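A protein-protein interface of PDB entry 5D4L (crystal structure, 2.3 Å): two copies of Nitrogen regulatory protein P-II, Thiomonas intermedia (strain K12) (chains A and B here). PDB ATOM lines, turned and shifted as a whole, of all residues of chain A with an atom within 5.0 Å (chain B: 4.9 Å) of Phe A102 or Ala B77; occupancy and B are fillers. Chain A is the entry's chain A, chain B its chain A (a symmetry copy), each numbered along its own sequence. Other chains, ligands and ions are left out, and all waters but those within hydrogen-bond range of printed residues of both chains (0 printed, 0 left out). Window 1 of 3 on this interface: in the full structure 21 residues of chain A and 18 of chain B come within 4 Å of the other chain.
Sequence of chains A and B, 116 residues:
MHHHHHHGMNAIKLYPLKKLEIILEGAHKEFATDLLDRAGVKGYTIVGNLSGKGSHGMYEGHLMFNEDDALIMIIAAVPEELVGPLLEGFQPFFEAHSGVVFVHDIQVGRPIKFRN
NZ of Lys B19 is in salt-bridge range of OE2 of Glu A21 (2.6 Å). A ring nitrogen (NE2) of His A56 lies within hydrogen-bond range of the backbone carbonyl oxygen (O) of Ile B75, at 2.9 Å. The backbone carbonyl oxygen of Gln B107 sits at hydrogen-bond distance from the backbone NH of Val A103.
NZ of Lys A19 is in salt-bridge range of OE1 of Glu A21. O of Lys A19 lies within hydrogen-bond range of N of His A104 (2.8 Å). The backbone NH of Glu A21 lies within hydrogen-bond range of the backbone carbonyl oxygen of Phe A102 (2.9 Å). The side-chain carboxylate of Glu A21 is in hydrogen-bond range of a ring nitrogen (NE2) of His A104 (3.2 Å). O of Ile B106 sits at hydrogen-bond distance from N of Leu B17 (3.1 Å).
Among the printed residues, merely in contact across the chains: His A56 with Ala B77 (3.9 Å), Gly A57 with Leu B17 (3.9 Å), Gly A57 with Val B108 (3.3 Å), Val A101 with Gln B107 (3.8 Å), Val A101 with Val B108 (3.9 Å), Phe A102 with Lys B19 (3.7 Å), Phe A102 with Ile B75 (3.98 Å), Phe A102 with Ala B77 (3.9 Å), Phe A102 with Ile B106 (3.5 Å), Phe A102 with Gln B107 (3.9 Å), Phe A102 with Val B108 (3.7 Å), Val A103 with Ile B106 (3.3 Å), His A104 with Lys B19 (3.3 Å) and His A104 with Ile B106 (3.5 Å).
Printed residues of chain B within 4 Å of Phe A102: Lys B19, Ile B75, Ala B77, Ile B106, Gln B107 and Val B108. Ala B77 touches two residues of chain A. Of the printed residues of chain A, Gln B107 touches Val A101 (3.8 Å), Phe A102 (3.9 Å) and Val A103 (3.0 Å). Printed residues of chain B within 4 Å of Gly A57: Leu B17 (3.9 Å) and Val B108 (3.3 Å). Printed residues of chain A within 4 Å of Lys B19: Glu A21, Phe A102 and His A104. Of the printed residues of chain B, Val A103 touches Ile B106 (3.3 Å) and Gln B107 (3.0 Å). Leu A20 touches none of the printed residues of chain B. The nearest printed residue of chain B that does not touch Val A103 is Val B108 (5.2 Å).
Position printed for both chains: 19.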
ATOM      1  N   LYS A  19     -12.276 -32.828  15.488  1.00  0.00           N
ATOM      2  CA  LYS A  19     -13.335 -33.677  14.955  1.00  0.00           C
ATOM      3  C   LYS A  19     -14.253 -32.864  14.064  1.00  0.00           C
ATOM      4  O   LYS A  19     -14.802 -31.855  14.479  1.00  0.00           O
ATOM      5  CB  LYS A  19     -14.158 -34.341  16.048  1.00  0.00           C
ATOM      6  CG  LYS A  19     -15.036 -35.474  15.502  1.00  0.00           C
ATOM      7  CD  LYS A  19     -16.095 -35.952  16.484  1.00  0.00           C
ATOM      8  CE  LYS A  19     -17.373 -35.194  16.332  1.00  0.00           C
ATOM      9  NZ  LYS A  19     -18.460 -35.703  17.257  1.00  0.00           N
ATOM     10  N   LEU A  20     -14.405 -33.343  12.842  1.00  0.00           N
ATOM     11  CA  LEU A  20     -15.190 -32.705  11.809  1.00  0.00           C
ATOM     12  C   LEU A  20     -16.499 -33.452  11.670  1.00  0.00           C
ATOM     13  O   LEU A  20     -16.491 -34.667  11.504  1.00  0.00           O
ATOM     14  CB  LEU A  20     -14.427 -32.724  10.482  1.00  0.00           C
ATOM     15  CG  LEU A  20     -13.521 -31.602   9.974  1.00  0.00           C
ATOM     16  CD1 LEU A  20     -12.842 -30.825  11.061  1.00  0.00           C
ATOM     17  CD2 LEU A  20     -12.469 -32.238   9.090  1.00  0.00           C
ATOM     18  N   GLU A  21     -17.617 -32.738  11.778  1.00  0.00           N
ATOM     19  CA  GLU A  21     -18.921 -33.292  11.440  1.00  0.00           C
ATOM     20  C   GLU A  21     -19.381 -32.634  10.149  1.00  0.00           C
ATOM     21  O   GLU A  21     -19.693 -31.447  10.129  1.00  0.00           O
ATOM     22  CB  GLU A  21     -19.932 -33.069  12.568  1.00  0.00           C
ATOM     23  CG  GLU A  21     -19.567 -33.805  13.865  1.00  0.00           C
ATOM     24  CD  GLU A  21     -20.539 -33.533  15.002  1.00  0.00           C
ATOM     25  OE1 GLU A  21     -20.533 -34.303  15.984  1.00  0.00           O
ATOM     26  OE2 GLU A  21     -21.318 -32.554  14.919  1.00  0.00           O
ATOM     27  N   ILE A  23     -22.030 -32.461   7.294  1.00  0.00           N
ATOM     28  CA  ILE A  23     -23.417 -32.774   7.005  1.00  0.00           C
ATOM     29  C   ILE A  23     -23.757 -32.306   5.595  1.00  0.00           C
ATOM     30  O   ILE A  23     -23.585 -31.148   5.277  1.00  0.00           O
ATOM     31  CB  ILE A  23     -24.367 -32.117   8.020  1.00  0.00           C
ATOM     32  CG1 ILE A  23     -23.985 -32.529   9.444  1.00  0.00           C
ATOM     33  CG2 ILE A  23     -25.815 -32.508   7.715  1.00  0.00           C
ATOM     34  CD1 ILE A  23     -24.499 -31.627  10.483  1.00  0.00           C
ATOM     35  N   HIS A  56     -27.563 -23.758   8.869  1.00  0.00           N
ATOM     36  CA  HIS A  56     -27.005 -24.479   9.991  1.00  0.00           C
ATOM     37  C   HIS A  56     -25.691 -23.865  10.444  1.00  0.00           C
ATOM     38  O   HIS A  56     -24.747 -24.582  10.756  1.00  0.00           O
ATOM     39  CB  HIS A  56     -26.820 -25.954   9.626  1.00  0.00           C
ATOM     40  CG  HIS A  56     -27.068 -26.893  10.766  1.00  0.00           C
ATOM     41  ND1 HIS A  56     -26.812 -28.247  10.690  1.00  0.00           N
ATOM     42  CD2 HIS A  56     -27.553 -26.672  12.011  1.00  0.00           C
ATOM     43  CE1 HIS A  56     -27.124 -28.818  11.842  1.00  0.00           C
ATOM     44  NE2 HIS A  56     -27.578 -27.885  12.659  1.00  0.00           N
ATOM     45  N   GLY A  57     -25.629 -22.534  10.461  1.00  0.00           N
ATOM     46  CA  GLY A  57     -24.473 -21.825  10.984  1.00  0.00           C
ATOM     47  C   GLY A  57     -23.585 -21.129   9.968  1.00  0.00           C
ATOM     48  O   GLY A  57     -22.579 -20.509  10.330  1.00  0.00           O
ATOM     49  N   VAL A 100     -22.800 -28.239   5.794  1.00  0.00           N
ATOM     50  CA  VAL A 100     -21.952 -27.534   6.742  1.00  0.00           C
ATOM     51  C   VAL A 100     -20.862 -28.465   7.315  1.00  0.00           C
ATOM     52  O   VAL A 100     -20.989 -29.702   7.262  1.00  0.00           O
ATOM     53  CB  VAL A 100     -22.815 -26.933   7.888  1.00  0.00           C
ATOM     54  CG1 VAL A 100     -23.392 -28.044   8.771  1.00  0.00           C
ATOM     55  CG2 VAL A 100     -22.034 -25.891   8.705  1.00  0.00           C
ATOM     56  N   VAL A 101     -19.791 -27.868   7.836  1.00  0.00           N
ATOM     57  CA  VAL A 101     -18.757 -28.592   8.578  1.00  0.00           C
ATOM     58  C   VAL A 101     -18.590 -27.971   9.955  1.00  0.00           C
ATOM     59  O   VAL A 101     -18.218 -26.798  10.080  1.00  0.00           O
ATOM     60  CB  VAL A 101     -17.390 -28.589   7.860  1.00  0.00           C
ATOM     61  CG1 VAL A 101     -16.349 -29.350   8.676  1.00  0.00           C
ATOM     62  CG2 VAL A 101     -17.512 -29.188   6.479  1.00  0.00           C
ATOM     63  N   PHE A 102     -18.900 -28.763  10.981  1.00  0.00           N
ATOM     64  CA  PHE A 102     -18.675 -28.401  12.375  1.00  0.00           C
ATOM     65  C   PHE A 102     -17.306 -28.880  12.812  1.00  0.00           C
ATOM     66  O   PHE A 102     -17.021 -30.074  12.747  1.00  0.00           O
ATOM     67  CB  PHE A 102     -19.735 -29.032  13.301  1.00  0.00           C
ATOM     68  CG  PHE A 102     -21.139 -28.569  13.043  1.00  0.00           C
ATOM     69  CD1 PHE A 102     -21.387 -27.329  12.488  1.00  0.00           C
ATOM     70  CD2 PHE A 102     -22.208 -29.369  13.371  1.00  0.00           C
ATOM     71  CE1 PHE A 102     -22.668 -26.900  12.264  1.00  0.00           C
ATOM     72  CE2 PHE A 102     -23.492 -28.940  13.150  1.00  0.00           C
ATOM     73  CZ  PHE A 102     -23.717 -27.709  12.586  1.00  0.00           C
ATOM     74  N   VAL A 103     -16.471 -27.962  13.272  1.00  0.00           N
ATOM     75  CA  VAL A 103     -15.157 -28.310  13.790  1.00  0.00           C
ATOM     76  C   VAL A 103     -15.177 -28.345  15.327  1.00  0.00           C
ATOM     77  O   VAL A 103     -15.557 -27.358  15.945  1.00  0.00           O
ATOM     78  CB  VAL A 103     -14.096 -27.299  13.293  1.00  0.00           C
ATOM     79  CG1 VAL A 103     -12.731 -27.620  13.871  1.00  0.00           C
ATOM     80  CG2 VAL A 103     -14.042 -27.297  11.778  1.00  0.00           C
ATOM     81  N   HIS A 104     -14.802 -29.480  15.934  1.00  0.00           N
ATOM     82  CA  HIS A 104     -14.706 -29.583  17.397  1.00  0.00           C
ATOM     83  C   HIS A 104     -13.253 -29.852  17.849  1.00  0.00           C
ATOM     84  O   HIS A 104     -12.449 -30.396  17.081  1.00  0.00           O
ATOM     85  CB  HIS A 104     -15.567 -30.721  17.981  1.00  0.00           C
ATOM     86  CG  HIS A 104     -16.958 -30.832  17.436  1.00  0.00           C
ATOM     87  ND1 HIS A 104     -18.077 -30.768  18.244  1.00  0.00           N
ATOM     88  CD2 HIS A 104     -17.415 -31.086  16.191  1.00  0.00           C
ATOM     89  CE1 HIS A 104     -19.161 -30.940  17.511  1.00  0.00           C
ATOM     90  NE2 HIS A 104     -18.787 -31.138  16.261  1.00  0.00           N
ATOM     91  N   LEU B  17     -19.285 -20.749  17.407  1.00  0.00           N
ATOM     92  CA  LEU B  17     -20.707 -20.899  17.669  1.00  0.00           C
ATOM     93  C   LEU B  17     -20.835 -21.923  18.781  1.00  0.00           C
ATOM     94  O   LEU B  17     -19.844 -22.545  19.152  1.00  0.00           O
ATOM     95  CB  LEU B  17     -21.470 -21.368  16.426  1.00  0.00           C
ATOM     96  CG  LEU B  17     -21.642 -20.441  15.225  1.00  0.00           C
ATOM     97  CD1 LEU B  17     -22.253 -21.239  14.116  1.00  0.00           C
ATOM     98  CD2 LEU B  17     -22.532 -19.281  15.559  1.00  0.00           C
ATOM     99  N   LYS B  18     -22.055 -22.098  19.283  1.00  0.00           N
ATOM    100  CA  LYS B  18     -22.393 -23.139  20.247  1.00  0.00           C
ATOM    101  C   LYS B  18     -23.167 -24.221  19.518  1.00  0.00           C
ATOM    102  O   LYS B  18     -24.079 -23.907  18.760  1.00  0.00           O
ATOM    103  CB  LYS B  18     -23.232 -22.575  21.397  1.00  0.00           C
ATOM    104  CG  LYS B  18     -22.516 -21.525  22.246  1.00  0.00           C
ATOM    105  CD  LYS B  18     -21.319 -22.176  22.930  1.00  0.00           C
ATOM    106  CE  LYS B  18     -20.739 -21.336  24.052  1.00  0.00           C
ATOM    107  NZ  LYS B  18     -19.520 -21.992  24.595  1.00  0.00           N
ATOM    108  N   LYS B  19     -22.805 -25.485  19.715  1.00  0.00           N
ATOM    109  CA  LYS B  19     -23.591 -26.564  19.129  1.00  0.00           C
ATOM    110  C   LYS B  19     -24.372 -27.285  20.211  1.00  0.00           C
ATOM    111  O   LYS B  19     -23.805 -27.764  21.181  1.00  0.00           O
ATOM    112  CB  LYS B  19     -22.735 -27.570  18.376  1.00  0.00           C
ATOM    113  CG  LYS B  19     -23.577 -28.500  17.493  1.00  0.00           C
ATOM    114  CD  LYS B  19     -22.810 -29.706  16.974  1.00  0.00           C
ATOM    115  CE  LYS B  19     -22.912 -30.871  17.905  1.00  0.00           C
ATOM    116  NZ  LYS B  19     -22.209 -32.102  17.369  1.00  0.00           N
ATOM    117  N   GLY B  43     -31.760 -22.767  11.700  1.00  0.00           N
ATOM    118  CA  GLY B  43     -31.940 -24.095  11.156  1.00  0.00           C
ATOM    119  C   GLY B  43     -31.498 -25.162  12.141  1.00  0.00           C
ATOM    120  O   GLY B  43     -30.931 -24.862  13.175  1.00  0.00           O
ATOM    121  N   ILE B  75     -29.936 -31.181  16.389  1.00  0.00           N
ATOM    122  CA  ILE B  75     -28.691 -30.424  16.419  1.00  0.00           C
ATOM    123  C   ILE B  75     -28.917 -28.982  15.913  1.00  0.00           C
ATOM    124  O   ILE B  75     -29.352 -28.772  14.786  1.00  0.00           O
ATOM    125  CB  ILE B  75     -27.588 -31.139  15.564  1.00  0.00           C
ATOM    126  CG1 ILE B  75     -27.369 -32.573  16.048  1.00  0.00           C
ATOM    127  CG2 ILE B  75     -26.277 -30.385  15.601  1.00  0.00           C
ATOM    128  CD1 ILE B  75     -26.391 -33.362  15.147  1.00  0.00           C
ATOM    129  N   ALA B  76     -28.629 -27.996  16.752  1.00  0.00           N
ATOM    130  CA  ALA B  76     -28.660 -26.604  16.333  1.00  0.00           C
ATOM    131  C   ALA B  76     -27.339 -25.907  16.637  1.00  0.00           C
ATOM    132  O   ALA B  76     -26.842 -25.968  17.761  1.00  0.00           O
ATOM    133  CB  ALA B  76     -29.772 -25.895  17.004  1.00  0.00           C
ATOM    134  N   ALA B  77     -26.768 -25.262  15.626  1.00  0.00           N
ATOM    135  CA  ALA B  77     -25.591 -24.424  15.812  1.00  0.00           C
ATOM    136  C   ALA B  77     -26.058 -22.971  15.931  1.00  0.00           C
ATOM    137  O   ALA B  77     -26.732 -22.447  15.050  1.00  0.00           O
ATOM    138  CB  ALA B  77     -24.630 -24.587  14.682  1.00  0.00           C
ATOM    139  N   VAL B  78     -25.645 -22.326  17.007  1.00  0.00           N
ATOM    140  CA  VAL B  78     -26.345 -21.191  17.565  1.00  0.00           C
ATOM    141  C   VAL B  78     -25.333 -20.194  18.150  1.00  0.00           C
ATOM    142  O   VAL B  78     -24.321 -20.610  18.725  1.00  0.00           O
ATOM    143  CB  VAL B  78     -27.359 -21.742  18.629  1.00  0.00           C
ATOM    144  CG1 VAL B  78     -27.098 -21.235  20.026  1.00  0.00           C
ATOM    145  CG2 VAL B  78     -28.779 -21.554  18.176  1.00  0.00           C
ATOM    146  N   PRO B  79     -25.571 -18.884  17.979  1.00  0.00           N
ATOM    147  CA  PRO B  79     -24.681 -17.902  18.612  1.00  0.00           C
ATOM    148  C   PRO B  79     -24.710 -18.067  20.125  1.00  0.00           C
ATOM    149  O   PRO B  79     -25.710 -18.525  20.632  1.00  0.00           O
ATOM    150  CB  PRO B  79     -25.280 -16.551  18.195  1.00  0.00           C
ATOM    151  CG  PRO B  79     -26.164 -16.858  17.028  1.00  0.00           C
ATOM    152  CD  PRO B  79     -26.681 -18.237  17.258  1.00  0.00           C
ATOM    153  N   ILE B 106     -18.019 -25.065  19.051  1.00  0.00           N
ATOM    154  CA  ILE B 106     -17.583 -25.473  17.729  1.00  0.00           C
ATOM    155  C   ILE B 106     -17.169 -24.263  16.935  1.00  0.00           C
ATOM    156  O   ILE B 106     -17.365 -23.132  17.377  1.00  0.00           O
ATOM    157  CB  ILE B 106     -18.667 -26.226  16.932  1.00  0.00           C
ATOM    158  CG1 ILE B 106     -19.821 -25.299  16.564  1.00  0.00           C
ATOM    159  CG2 ILE B 106     -19.144 -27.445  17.693  1.00  0.00           C
ATOM    160  CD1 ILE B 106     -20.830 -25.917  15.605  1.00  0.00           C
ATOM    161  N   GLN B 107     -16.591 -24.508  15.765  1.00  0.00           N
ATOM    162  CA  GLN B 107     -16.298 -23.436  14.834  1.00  0.00           C
ATOM    163  C   GLN B 107     -16.815 -23.825  13.470  1.00  0.00           C
ATOM    164  O   GLN B 107     -16.858 -25.013  13.156  1.00  0.00           O
ATOM    165  CB  GLN B 107     -14.798 -23.144  14.793  1.00  0.00           C
ATOM    166  CG  GLN B 107     -14.242 -22.814  16.185  1.00  0.00           C
ATOM    167  CD  GLN B 107     -12.811 -22.327  16.159  1.00  0.00           C
ATOM    168  OE1 GLN B 107     -12.075 -22.566  15.200  1.00  0.00           O
ATOM    169  NE2 GLN B 107     -12.407 -21.631  17.215  1.00  0.00           N
ATOM    170  N   VAL B 108     -17.223 -22.831  12.676  1.00  0.00           N
ATOM    171  CA  VAL B 108     -17.662 -23.058  11.309  1.00  0.00           C
ATOM    172  C   VAL B 108     -16.913 -22.114  10.369  1.00  0.00           C
ATOM    173  O   VAL B 108     -16.729 -20.928  10.656  1.00  0.00           O
ATOM    174  CB  VAL B 108     -19.199 -22.876  11.141  1.00  0.00           C
ATOM    175  CG1 VAL B 108     -19.952 -23.905  11.961  1.00  0.00           C
ATOM    176  CG2 VAL B 108     -19.636 -21.486  11.540  1.00  0.00           C
